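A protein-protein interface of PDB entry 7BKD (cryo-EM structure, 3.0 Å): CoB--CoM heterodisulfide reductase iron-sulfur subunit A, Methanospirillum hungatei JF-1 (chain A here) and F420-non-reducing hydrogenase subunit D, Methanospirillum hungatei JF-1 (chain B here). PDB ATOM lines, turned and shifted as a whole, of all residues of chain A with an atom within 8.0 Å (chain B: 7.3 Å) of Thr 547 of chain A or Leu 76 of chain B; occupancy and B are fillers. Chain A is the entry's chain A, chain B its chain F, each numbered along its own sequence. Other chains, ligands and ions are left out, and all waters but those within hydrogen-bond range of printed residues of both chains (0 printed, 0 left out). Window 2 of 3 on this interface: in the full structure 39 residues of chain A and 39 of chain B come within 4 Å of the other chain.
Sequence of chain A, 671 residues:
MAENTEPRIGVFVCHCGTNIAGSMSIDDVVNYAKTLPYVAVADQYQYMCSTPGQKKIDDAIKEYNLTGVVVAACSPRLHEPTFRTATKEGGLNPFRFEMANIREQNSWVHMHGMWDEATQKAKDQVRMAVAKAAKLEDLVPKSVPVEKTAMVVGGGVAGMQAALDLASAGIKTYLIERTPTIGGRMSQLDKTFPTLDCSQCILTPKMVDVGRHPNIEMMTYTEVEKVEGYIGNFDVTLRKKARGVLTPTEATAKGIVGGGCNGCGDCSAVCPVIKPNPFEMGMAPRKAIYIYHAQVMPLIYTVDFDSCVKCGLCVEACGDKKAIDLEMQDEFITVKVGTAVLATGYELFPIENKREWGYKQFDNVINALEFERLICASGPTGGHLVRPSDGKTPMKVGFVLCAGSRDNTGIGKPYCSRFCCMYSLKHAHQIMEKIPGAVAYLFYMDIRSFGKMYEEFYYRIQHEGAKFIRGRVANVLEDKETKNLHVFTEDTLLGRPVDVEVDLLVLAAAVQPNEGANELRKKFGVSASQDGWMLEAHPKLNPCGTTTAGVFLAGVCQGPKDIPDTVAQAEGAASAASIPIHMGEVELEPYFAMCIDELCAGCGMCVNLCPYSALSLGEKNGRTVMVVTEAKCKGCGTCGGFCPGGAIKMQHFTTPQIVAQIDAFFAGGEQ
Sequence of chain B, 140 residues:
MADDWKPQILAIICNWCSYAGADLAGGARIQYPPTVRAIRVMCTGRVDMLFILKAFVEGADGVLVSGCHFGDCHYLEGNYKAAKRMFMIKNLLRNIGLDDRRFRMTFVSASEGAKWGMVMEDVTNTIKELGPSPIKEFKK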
ATOM      1  N   PHE A 524       7.324  -0.646  11.465  1.00  0.00           N
ATOM      2  CA  PHE A 524       7.113  -2.048  11.797  1.00  0.00           C
ATOM      3  C   PHE A 524       7.139  -2.306  13.298  1.00  0.00           C
ATOM      4  O   PHE A 524       7.082  -3.465  13.716  1.00  0.00           O
ATOM      5  CB  PHE A 524       8.165  -2.918  11.110  1.00  0.00           C
ATOM      6  CG  PHE A 524       7.799  -3.328   9.716  1.00  0.00           C
ATOM      7  CD1 PHE A 524       6.966  -4.408   9.496  1.00  0.00           C
ATOM      8  CD2 PHE A 524       8.293  -2.637   8.626  1.00  0.00           C
ATOM      9  CE1 PHE A 524       6.629  -4.788   8.214  1.00  0.00           C
ATOM     10  CE2 PHE A 524       7.960  -3.012   7.343  1.00  0.00           C
ATOM     11  CZ  PHE A 524       7.128  -4.089   7.137  1.00  0.00           C
ATOM     12  N   GLY A 525       7.224  -1.259  14.111  1.00  0.00           N
ATOM     13  CA  GLY A 525       7.291  -1.424  15.553  1.00  0.00           C
ATOM     14  C   GLY A 525       8.558  -2.080  16.058  1.00  0.00           C
ATOM     15  O   GLY A 525       8.516  -2.814  17.052  1.00  0.00           O
ATOM     16  N   VAL A 526       9.688  -1.823  15.408  1.00  0.00           N
ATOM     17  CA  VAL A 526      10.978  -2.367  15.815  1.00  0.00           C
ATOM     18  C   VAL A 526      11.765  -1.269  16.510  1.00  0.00           C
ATOM     19  O   VAL A 526      11.893  -0.159  15.982  1.00  0.00           O
ATOM     20  CB  VAL A 526      11.755  -2.919  14.609  1.00  0.00           C
ATOM     21  CG1 VAL A 526      13.085  -3.497  15.057  1.00  0.00           C
ATOM     22  CG2 VAL A 526      10.931  -3.966  13.886  1.00  0.00           C
ATOM     23  N   SER A 527      12.286  -1.571  17.694  1.00  0.00           N
ATOM     24  CA  SER A 527      13.057  -0.591  18.442  1.00  0.00           C
ATOM     25  C   SER A 527      14.498  -0.556  17.952  1.00  0.00           C
ATOM     26  O   SER A 527      15.043  -1.556  17.481  1.00  0.00           O
ATOM     27  CB  SER A 527      13.030  -0.905  19.937  1.00  0.00           C
ATOM     28  OG  SER A 527      13.700  -2.121  20.213  1.00  0.00           O
ATOM     29  N   LEU A 535      17.246  -3.242  16.938  1.00  0.00           N
ATOM     30  CA  LEU A 535      17.463  -4.064  18.119  1.00  0.00           C
ATOM     31  C   LEU A 535      16.994  -5.495  17.884  1.00  0.00           C
ATOM     32  O   LEU A 535      16.114  -5.758  17.060  1.00  0.00           O
ATOM     33  CB  LEU A 535      16.736  -3.468  19.324  1.00  0.00           C
ATOM     34  CG  LEU A 535      17.150  -3.999  20.695  1.00  0.00           C
ATOM     35  CD1 LEU A 535      18.661  -4.000  20.827  1.00  0.00           C
ATOM     36  CD2 LEU A 535      16.509  -3.184  21.800  1.00  0.00           C
ATOM     37  N   GLU A 536      17.584  -6.420  18.631  1.00  0.00           N
ATOM     38  CA  GLU A 536      17.331  -7.843  18.475  1.00  0.00           C
ATOM     39  C   GLU A 536      16.406  -8.336  19.578  1.00  0.00           C
ATOM     40  O   GLU A 536      16.290  -7.724  20.643  1.00  0.00           O
ATOM     41  CB  GLU A 536      18.641  -8.624  18.521  1.00  0.00           C
ATOM     42  CG  GLU A 536      19.474  -8.461  17.281  1.00  0.00           C
ATOM     43  CD  GLU A 536      20.344  -7.221  17.372  1.00  0.00           C
ATOM     44  OE1 GLU A 536      21.155  -7.134  18.318  1.00  0.00           O
ATOM     45  OE2 GLU A 536      20.208  -6.325  16.517  1.00  0.00           O
ATOM     46  N   ALA A 537      15.746  -9.463  19.313  1.00  0.00           N
ATOM     47  CA  ALA A 537      14.920 -10.086  20.341  1.00  0.00           C
ATOM     48  C   ALA A 537      15.767 -10.526  21.527  1.00  0.00           C
ATOM     49  O   ALA A 537      15.364 -10.365  22.684  1.00  0.00           O
ATOM     50  CB  ALA A 537      14.152 -11.269  19.754  1.00  0.00           C
ATOM     51  N   HIS A 538      16.946 -11.085  21.258  1.00  0.00           N
ATOM     52  CA  HIS A 538      17.893 -11.438  22.285  1.00  0.00           C
ATOM     53  C   HIS A 538      19.274 -11.302  21.663  1.00  0.00           C
ATOM     54  O   HIS A 538      19.521 -11.901  20.605  1.00  0.00           O
ATOM     55  CB  HIS A 538      17.692 -12.853  22.818  1.00  0.00           C
ATOM     56  CG  HIS A 538      18.412 -13.119  24.101  1.00  0.00           C
ATOM     57  ND1 HIS A 538      19.756 -13.418  24.150  1.00  0.00           N
ATOM     58  CD2 HIS A 538      17.977 -13.131  25.382  1.00  0.00           C
ATOM     59  CE1 HIS A 538      20.118 -13.602  25.407  1.00  0.00           C
ATOM     60  NE2 HIS A 538      19.056 -13.434  26.174  1.00  0.00           N
ATOM     61  N   PRO A 539      20.177 -10.536  22.275  1.00  0.00           N
ATOM     62  CA  PRO A 539      21.495 -10.319  21.657  1.00  0.00           C
ATOM     63  C   PRO A 539      22.310 -11.585  21.487  1.00  0.00           C
ATOM     64  O   PRO A 539      23.207 -11.613  20.638  1.00  0.00           O
ATOM     65  CB  PRO A 539      22.178  -9.343  22.626  1.00  0.00           C
ATOM     66  CG  PRO A 539      21.058  -8.696  23.366  1.00  0.00           C
ATOM     67  CD  PRO A 539      20.018  -9.759  23.514  1.00  0.00           C
ATOM     68  N   ASN A 542      19.054 -15.134  19.852  1.00  0.00           N
ATOM     69  CA  ASN A 542      18.095 -14.825  18.791  1.00  0.00           C
ATOM     70  C   ASN A 542      18.593 -13.614  18.015  1.00  0.00           C
ATOM     71  O   ASN A 542      17.996 -12.532  18.063  1.00  0.00           O
ATOM     72  CB  ASN A 542      16.704 -14.576  19.370  1.00  0.00           C
ATOM     73  CG  ASN A 542      15.610 -14.727  18.339  1.00  0.00           C
ATOM     74  OD1 ASN A 542      15.869 -14.733  17.137  1.00  0.00           O
ATOM     75  ND2 ASN A 542      14.374 -14.848  18.803  1.00  0.00           N
ATOM     76  N   CYS A 544      18.394 -13.024  14.946  1.00  0.00           N
ATOM     77  CA  CYS A 544      17.548 -12.699  13.808  1.00  0.00           C
ATOM     78  C   CYS A 544      16.214 -12.089  14.212  1.00  0.00           C
ATOM     79  O   CYS A 544      15.641 -11.310  13.443  1.00  0.00           O
ATOM     80  CB  CYS A 544      17.296 -13.955  12.970  1.00  0.00           C
ATOM     81  SG  CYS A 544      18.771 -14.951  12.659  1.00  0.00           S
ATOM     82  N   GLY A 545      15.710 -12.418  15.396  1.00  0.00           N
ATOM     83  CA  GLY A 545      14.373 -12.035  15.783  1.00  0.00           C
ATOM     84  C   GLY A 545      14.265 -10.604  16.269  1.00  0.00           C
ATOM     85  O   GLY A 545      15.218  -9.828  16.271  1.00  0.00           O
ATOM     86  N   THR A 546      13.052 -10.260  16.688  1.00  0.00           N
ATOM     87  CA  THR A 546      12.730  -8.934  17.189  1.00  0.00           C
ATOM     88  C   THR A 546      11.617  -9.100  18.214  1.00  0.00           C
ATOM     89  O   THR A 546      10.908 -10.108  18.220  1.00  0.00           O
ATOM     90  CB  THR A 546      12.318  -7.999  16.039  1.00  0.00           C
ATOM     91  OG1 THR A 546      13.398  -7.894  15.105  1.00  0.00           O
ATOM     92  CG2 THR A 546      11.994  -6.605  16.536  1.00  0.00           C
ATOM     93  N   THR A 547      11.479  -8.111  19.099  1.00  0.00           N
ATOM     94  CA  THR A 547      10.417  -8.170  20.097  1.00  0.00           C
ATOM     95  C   THR A 547       9.046  -8.234  19.439  1.00  0.00           C
ATOM     96  O   THR A 547       8.168  -8.975  19.894  1.00  0.00           O
ATOM     97  CB  THR A 547      10.505  -6.970  21.038  1.00  0.00           C
ATOM     98  OG1 THR A 547      10.370  -5.759  20.283  1.00  0.00           O
ATOM     99  CG2 THR A 547      11.838  -6.966  21.766  1.00  0.00           C
ATOM    100  N   THR A 548       8.838  -7.470  18.371  1.00  0.00           N
ATOM    101  CA  THR A 548       7.594  -7.584  17.623  1.00  0.00           C
ATOM    102  C   THR A 548       7.562  -8.908  16.868  1.00  0.00           C
ATOM    103  O   THR A 548       8.535  -9.294  16.215  1.00  0.00           O
ATOM    104  CB  THR A 548       7.419  -6.398  16.670  1.00  0.00           C
ATOM    105  OG1 THR A 548       6.149  -6.488  16.016  1.00  0.00           O
ATOM    106  CG2 THR A 548       8.520  -6.341  15.636  1.00  0.00           C
ATOM    107  N   ALA A 549       6.449  -9.623  16.989  1.00  0.00           N
ATOM    108  CA  ALA A 549       6.345 -10.947  16.398  1.00  0.00           C
ATOM    109  C   ALA A 549       6.209 -10.856  14.885  1.00  0.00           C
ATOM    110  O   ALA A 549       5.622  -9.916  14.345  1.00  0.00           O
ATOM    111  CB  ALA A 549       5.154 -11.700  16.985  1.00  0.00           C
ATOM    112  N   GLY A 550       6.769 -11.847  14.199  1.00  0.00           N
ATOM    113  CA  GLY A 550       6.654 -11.932  12.761  1.00  0.00           C
ATOM    114  C   GLY A 550       7.559 -11.009  11.980  1.00  0.00           C
ATOM    115  O   GLY A 550       7.444 -10.957  10.751  1.00  0.00           O
ATOM    116  N   VAL A 551       8.449 -10.279  12.642  1.00  0.00           N
ATOM    117  CA  VAL A 551       9.402  -9.400  11.978  1.00  0.00           C
ATOM    118  C   VAL A 551      10.802  -9.879  12.325  1.00  0.00           C
ATOM    119  O   VAL A 551      11.108 -10.120  13.497  1.00  0.00           O
ATOM    120  CB  VAL A 551       9.203  -7.930  12.386  1.00  0.00           C
ATOM    121  CG1 VAL A 551      10.163  -7.038  11.623  1.00  0.00           C
ATOM    122  CG2 VAL A 551       7.771  -7.506  12.134  1.00  0.00           C
ATOM    123  N   LEU A 553      15.206  -9.663  11.242  1.00  0.00           N
ATOM    124  CA  LEU A 553      16.245  -8.776  10.745  1.00  0.00           C
ATOM    125  C   LEU A 553      17.322  -9.570  10.024  1.00  0.00           C
ATOM    126  O   LEU A 553      17.667 -10.682  10.435  1.00  0.00           O
ATOM    127  CB  LEU A 553      16.873  -7.979  11.888  1.00  0.00           C
ATOM    128  CG  LEU A 553      15.897  -7.238  12.796  1.00  0.00           C
ATOM    129  CD1 LEU A 553      16.623  -6.699  14.011  1.00  0.00           C
ATOM    130  CD2 LEU A 553      15.205  -6.121  12.035  1.00  0.00           C
ATOM    131  N   PRO A 611       5.703  -4.675  27.011  1.00  0.00           N
ATOM    132  CA  PRO A 611       6.905  -4.585  26.173  1.00  0.00           C
ATOM    133  C   PRO A 611       6.666  -4.964  24.727  1.00  0.00           C
ATOM    134  O   PRO A 611       7.427  -4.532  23.855  1.00  0.00           O
ATOM    135  CB  PRO A 611       7.880  -5.560  26.847  1.00  0.00           C
ATOM    136  CG  PRO A 611       7.268  -5.901  28.165  1.00  0.00           C
ATOM    137  CD  PRO A 611       5.808  -5.744  28.012  1.00  0.00           C
ATOM    138  N   TYR A 612       5.636  -5.755  24.440  1.00  0.00           N
ATOM    139  CA  TYR A 612       5.416  -6.301  23.113  1.00  0.00           C
ATOM    140  C   TYR A 612       4.329  -5.575  22.339  1.00  0.00           C
ATOM    141  O   TYR A 612       3.949  -6.031  21.258  1.00  0.00           O
ATOM    142  CB  TYR A 612       5.086  -7.787  23.216  1.00  0.00           C
ATOM    143  CG  TYR A 612       6.140  -8.567  23.955  1.00  0.00           C
ATOM    144  CD1 TYR A 612       7.310  -8.950  23.325  1.00  0.00           C
ATOM    145  CD2 TYR A 612       5.975  -8.906  25.284  1.00  0.00           C
ATOM    146  CE1 TYR A 612       8.277  -9.655  23.993  1.00  0.00           C
ATOM    147  CE2 TYR A 612       6.939  -9.613  25.961  1.00  0.00           C
ATOM    148  CZ  TYR A 612       8.086  -9.984  25.309  1.00  0.00           C
ATOM    149  OH  TYR A 612       9.053 -10.690  25.978  1.00  0.00           O
ATOM    150  N   SER A 613       3.821  -4.462  22.866  1.00  0.00           N
ATOM    151  CA  SER A 613       2.818  -3.647  22.182  1.00  0.00           C
ATOM    152  C   SER A 613       1.575  -4.458  21.835  1.00  0.00           C
ATOM    153  O   SER A 613       0.944  -4.249  20.800  1.00  0.00           O
ATOM    154  CB  SER A 613       3.401  -2.991  20.932  1.00  0.00           C
ATOM    155  OG  SER A 613       4.430  -2.081  21.271  1.00  0.00           O
ATOM    156  N   ALA A 631      -1.935 -12.693  19.712  1.00  0.00           N
ATOM    157  CA  ALA A 631      -0.738 -13.137  19.013  1.00  0.00           C
ATOM    158  C   ALA A 631       0.526 -12.506  19.572  1.00  0.00           C
ATOM    159  O   ALA A 631       1.613 -13.058  19.382  1.00  0.00           O
ATOM    160  CB  ALA A 631      -0.856 -12.827  17.524  1.00  0.00           C
ATOM    161  N   LYS A 632       0.413 -11.369  20.255  1.00  0.00           N
ATOM    162  CA  LYS A 632       1.575 -10.685  20.805  1.00  0.00           C
ATOM    163  C   LYS A 632       1.766 -10.907  22.297  1.00  0.00           C
ATOM    164  O   LYS A 632       2.900 -10.830  22.776  1.00  0.00           O
ATOM    165  CB  LYS A 632       1.482  -9.181  20.543  1.00  0.00           C
ATOM    166  CG  LYS A 632       1.600  -8.774  19.097  1.00  0.00           C
ATOM    167  CD  LYS A 632       1.524  -7.267  18.984  1.00  0.00           C
ATOM    168  CE  LYS A 632       1.616  -6.802  17.552  1.00  0.00           C
ATOM    169  NZ  LYS A 632       1.528  -5.322  17.463  1.00  0.00           N
ATOM    170  N   LYS A 634       2.385 -12.539  25.895  1.00  0.00           N
ATOM    171  CA  LYS A 634       3.259 -13.634  26.287  1.00  0.00           C
ATOM    172  C   LYS A 634       3.014 -14.096  27.714  1.00  0.00           C
ATOM    173  O   LYS A 634       3.831 -14.844  28.256  1.00  0.00           O
ATOM    174  CB  LYS A 634       4.722 -13.234  26.111  1.00  0.00           C
ATOM    175  CG  LYS A 634       5.166 -13.273  24.673  1.00  0.00           C
ATOM    176  CD  LYS A 634       6.664 -13.292  24.553  1.00  0.00           C
ATOM    177  CE  LYS A 634       7.075 -13.095  23.114  1.00  0.00           C
ATOM    178  NZ  LYS A 634       6.490 -14.153  22.250  1.00  0.00           N
ATOM    179  N   CYS A 636       3.182 -12.460  30.489  1.00  0.00           N
ATOM    180  CA  CYS A 636       4.052 -11.878  31.503  1.00  0.00           C
ATOM    181  C   CYS A 636       3.264 -11.487  32.742  1.00  0.00           C
ATOM    182  O   CYS A 636       3.693 -11.752  33.868  1.00  0.00           O
ATOM    183  CB  CYS A 636       4.792 -10.675  30.927  1.00  0.00           C
ATOM    184  SG  CYS A 636       3.882  -9.141  30.981  1.00  0.00           S
ATOM    185  N   THR A 638       2.201  -8.242  33.421  1.00  0.00           N
ATOM    186  CA  THR A 638       2.449  -6.879  33.874  1.00  0.00           C
ATOM    187  C   THR A 638       1.167  -6.062  33.883  1.00  0.00           C
ATOM    188  O   THR A 638       0.880  -5.347  34.847  1.00  0.00           O
ATOM    189  CB  THR A 638       3.496  -6.214  32.984  1.00  0.00           C
ATOM    190  OG1 THR A 638       4.730  -6.932  33.083  1.00  0.00           O
ATOM    191  CG2 THR A 638       3.721  -4.786  33.405  1.00  0.00           C
ATOM    192  N   CYS B  43       6.232 -13.596  36.319  1.00  0.00           N
ATOM    193  CA  CYS B  43       7.219 -12.570  36.004  1.00  0.00           C
ATOM    194  C   CYS B  43       7.481 -11.538  37.090  1.00  0.00           C
ATOM    195  O   CYS B  43       8.199 -10.577  36.815  1.00  0.00           O
ATOM    196  CB  CYS B  43       6.811 -11.821  34.724  1.00  0.00           C
ATOM    197  SG  CYS B  43       8.081 -10.734  34.000  1.00  0.00           S
ATOM    198  N   GLY B  71      17.639  -6.110  33.376  1.00  0.00           N
ATOM    199  CA  GLY B  71      18.138  -6.530  32.088  1.00  0.00           C
ATOM    200  C   GLY B  71      18.118  -8.023  31.854  1.00  0.00           C
ATOM    201  O   GLY B  71      18.535  -8.468  30.779  1.00  0.00           O
ATOM    202  N   ASP B  72      17.643  -8.811  32.818  1.00  0.00           N
ATOM    203  CA  ASP B  72      17.608 -10.260  32.692  1.00  0.00           C
ATOM    204  C   ASP B  72      16.202 -10.828  32.803  1.00  0.00           C
ATOM    205  O   ASP B  72      16.050 -12.044  32.958  1.00  0.00           O
ATOM    206  CB  ASP B  72      18.505 -10.910  33.745  1.00  0.00           C
ATOM    207  CG  ASP B  72      19.971 -10.616  33.522  1.00  0.00           C
ATOM    208  OD1 ASP B  72      20.763 -10.788  34.471  1.00  0.00           O
ATOM    209  OD2 ASP B  72      20.331 -10.213  32.396  1.00  0.00           O
ATOM    210  N   CYS B  73      15.172  -9.989  32.739  1.00  0.00           N
ATOM    211  CA  CYS B  73      13.805 -10.480  32.825  1.00  0.00           C
ATOM    212  C   CYS B  73      13.463 -11.309  31.597  1.00  0.00           C
ATOM    213  O   CYS B  73      13.864 -10.985  30.478  1.00  0.00           O
ATOM    214  CB  CYS B  73      12.826  -9.315  32.956  1.00  0.00           C
ATOM    215  SG  CYS B  73      11.130  -9.798  33.327  1.00  0.00           S
ATOM    216  N   HIS B  74      12.716 -12.391  31.814  1.00  0.00           N
ATOM    217  CA  HIS B  74      12.316 -13.236  30.698  1.00  0.00           C
ATOM    218  C   HIS B  74      11.389 -12.501  29.743  1.00  0.00           C
ATOM    219  O   HIS B  74      11.352 -12.820  28.550  1.00  0.00           O
ATOM    220  CB  HIS B  74      11.651 -14.504  31.218  1.00  0.00           C
ATOM    221  CG  HIS B  74      11.327 -15.499  30.150  1.00  0.00           C
ATOM    222  ND1 HIS B  74      12.290 -16.265  29.532  1.00  0.00           N
ATOM    223  CD2 HIS B  74      10.147 -15.865  29.601  1.00  0.00           C
ATOM    224  CE1 HIS B  74      11.717 -17.053  28.642  1.00  0.00           C
ATOM    225  NE2 HIS B  74      10.416 -16.830  28.665  1.00  0.00           N
ATOM    226  N   TYR B  75      10.641 -11.518  30.241  1.00  0.00           N
ATOM    227  CA  TYR B  75       9.716 -10.734  29.436  1.00  0.00           C
ATOM    228  C   TYR B  75      10.188  -9.295  29.262  1.00  0.00           C
ATOM    229  O   TYR B  75       9.388  -8.415  28.940  1.00  0.00           O
ATOM    230  CB  TYR B  75       8.325 -10.787  30.052  1.00  0.00           C
ATOM    231  CG  TYR B  75       7.809 -12.193  30.237  1.00  0.00           C
ATOM    232  CD1 TYR B  75       7.224 -12.878  29.191  1.00  0.00           C
ATOM    233  CD2 TYR B  75       7.911 -12.834  31.454  1.00  0.00           C
ATOM    234  CE1 TYR B  75       6.754 -14.155  29.356  1.00  0.00           C
ATOM    235  CE2 TYR B  75       7.442 -14.108  31.628  1.00  0.00           C
ATOM    236  CZ  TYR B  75       6.866 -14.764  30.577  1.00  0.00           C
ATOM    237  OH  TYR B  75       6.398 -16.041  30.748  1.00  0.00           O
ATOM    238  N   LEU B  76      11.465  -9.045  29.530  1.00  0.00           N
ATOM    239  CA  LEU B  76      12.228  -7.871  29.118  1.00  0.00           C
ATOM    240  C   LEU B  76      11.936  -6.583  29.875  1.00  0.00           C
ATOM    241  O   LEU B  76      12.752  -5.659  29.828  1.00  0.00           O
ATOM    242  CB  LEU B  76      11.987  -7.598  27.633  1.00  0.00           C
ATOM    243  CG  LEU B  76      12.672  -8.449  26.575  1.00  0.00           C
ATOM    244  CD1 LEU B  76      11.891  -8.349  25.283  1.00  0.00           C
ATOM    245  CD2 LEU B  76      14.101  -7.994  26.367  1.00  0.00           C
ATOM    246  N   GLU B  77      10.828  -6.498  30.595  1.00  0.00           N
ATOM    247  CA  GLU B  77      10.551  -5.260  31.315  1.00  0.00           C
ATOM    248  C   GLU B  77       9.834  -5.446  32.641  1.00  0.00           C
ATOM    249  O   GLU B  77       9.565  -4.445  33.305  1.00  0.00           O
ATOM    250  CB  GLU B  77       9.723  -4.311  30.431  1.00  0.00           C
ATOM    251  CG  GLU B  77      10.453  -3.703  29.241  1.00  0.00           C
ATOM    252  CD  GLU B  77      11.475  -2.660  29.642  1.00  0.00           C
ATOM    253  OE1 GLU B  77      11.077  -1.621  30.209  1.00  0.00           O
ATOM    254  OE2 GLU B  77      12.678  -2.874  29.386  1.00  0.00           O
ATOM    255  N   GLY B  78       9.518  -6.669  33.061  1.00  0.00           N
ATOM    256  CA  GLY B  78       8.607  -6.835  34.182  1.00  0.00           C
ATOM    257  C   GLY B  78       9.188  -6.379  35.503  1.00  0.00           C
ATOM    258  O   GLY B  78       8.486  -5.798  36.336  1.00  0.00           O
ATOM    259  N   ASN B  79      10.472  -6.645  35.722  1.00  0.00           N
ATOM    260  CA  ASN B  79      11.061  -6.350  37.016  1.00  0.00           C
ATOM    261  C   ASN B  79      11.196  -4.856  37.267  1.00  0.00           C
ATOM    262  O   ASN B  79      11.263  -4.449  38.424  1.00  0.00           O
ATOM    263  CB  ASN B  79      12.410  -7.056  37.150  1.00  0.00           C
ATOM    264  CG  ASN B  79      13.316  -6.811  35.974  1.00  0.00           C
ATOM    265  OD1 ASN B  79      12.992  -6.046  35.072  1.00  0.00           O
ATOM    266  ND2 ASN B  79      14.463  -7.468  35.972  1.00  0.00           N
ATOM    267  N   TYR B  80      11.187  -4.024  36.226  1.00  0.00           N
ATOM    268  CA  TYR B  80      11.197  -2.582  36.455  1.00  0.00           C
ATOM    269  C   TYR B  80       9.851  -2.093  36.972  1.00  0.00           C
ATOM    270  O   TYR B  80       9.792  -1.266  37.892  1.00  0.00           O
ATOM    271  CB  TYR B  80      11.583  -1.860  35.171  1.00  0.00           C
ATOM    272  CG  TYR B  80      12.827  -2.423  34.553  1.00  0.00           C
ATOM    273  CD1 TYR B  80      14.067  -2.201  35.125  1.00  0.00           C
ATOM    274  CD2 TYR B  80      12.764  -3.194  33.411  1.00  0.00           C
ATOM    275  CE1 TYR B  80      15.208  -2.721  34.571  1.00  0.00           C
ATOM    276  CE2 TYR B  80      13.901  -3.723  32.850  1.00  0.00           C
ATOM    277  CZ  TYR B  80      15.120  -3.483  33.434  1.00  0.00           C
ATOM    278  OH  TYR B  80      16.257  -4.005  32.871  1.00  0.00           O
ATOM    279  N   LYS B  81       8.759  -2.587  36.391  1.00  0.00           N
ATOM    280  CA  LYS B  81       7.438  -2.288  36.930  1.00  0.00           C
ATOM    281  C   LYS B  81       7.316  -2.795  38.357  1.00  0.00           C
ATOM    282  O   LYS B  81       6.782  -2.103  39.234  1.00  0.00           O
ATOM    283  CB  LYS B  81       6.365  -2.914  36.044  1.00  0.00           C
ATOM    284  CG  LYS B  81       6.028  -2.099  34.819  1.00  0.00           C
ATOM    285  CD  LYS B  81       6.923  -2.447  33.660  1.00  0.00           C
ATOM    286  CE  LYS B  81       6.579  -1.611  32.453  1.00  0.00           C
ATOM    287  NZ  LYS B  81       7.452  -1.914  31.296  1.00  0.00           N
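Among the printed residues, merely in contact across the chains: Lys 634 of chain A with Tyr 75 of chain B (3.2 Å), Cys 636 of chain A with Cys 43 of chain B (3.2 Å), Pro 611 of chain A with Tyr 75 of chain B (3.4 Å), Cys 636 of chain A with Tyr 75 of chain B (3.4 Å), Tyr 612 of chain A with Tyr 75 of chain B (3.5 Å), Pro 611 of chain A with Glu 77 of chain B (3.7 Å), Tyr 612 of chain A with Leu 76 of chain B (3.7 Å), Thr 547 of chain A with Leu 76 of chain B (3.8 Å) and Thr 638 of chain A with Lys 81 of chain B (3.8 Å).
Leu 76 of chain B touches just these residues of chain A: Thr 547 and Tyr 612.
Of the printed residues of chain B, Thr 638 of chain A touches Lys 81 (3.8 Å).
Of the printed residues of chain B, Pro 611 of chain A touches Tyr 75 (3.4 Å) and Glu 77 (3.7 Å).
Printed residues of chain B within 4 Å of Tyr 612 of chain A: Tyr 75 and Leu 76.
Printed residues of chain A within 4 Å of Cys 43 of chain B: Cys 636.
Of the printed residues of chain A, Lys 81 of chain B touches Thr 638 (3.8 Å).
Ala 631 of chain A touches none of the printed residues of chain B.
Gly 78 of chain B touches none of the printed residues of chain A.
The nearest printed residue of chain B that does not touch Thr 547 of chain A is Tyr 75 of chain B (7.7 Å).
The nearest residue of chain A that does not touch Leu 76 of chain B is Ala 537 of chain A (4.6 Å).
The nearest printed residue of chain A that does not touch Lys 81 of chain B is Pro 611 of chain A (5.1 Å).
The side-chain sulfur (SG) of Cys 636 of chain A sits close to the backbone NH (N) of Thr 638 of chain A.
N of Tyr 75 of chain B lies close to SG of Cys 73 of chain B.
The side-chain amino group (NZ) of Lys 81 of chain B lies within salt-bridge range of the side-chain carboxylate (OE1) of Glu 77 of chain B (3.8 Å).
Printed residues of chain A that touch a printed residue of chain B: Thr 547, Pro 611, Tyr 612, Lys 634, Cys 636 and Thr 638.
Hydrophobic or aromatic side chains of chain A within 4 Å of the printed part of chain B: Pro 611 and Tyr 612.
Along chain B the printed residues that touch a printed residue of chain A span positions 43 to 81.
Among the printed residues, 9 pairs touch across the chains.
Among the printed residues, no Asp or Glu carboxylate lies within 4 Å of a Lys or Arg side-chain nitrogen of the other chain.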
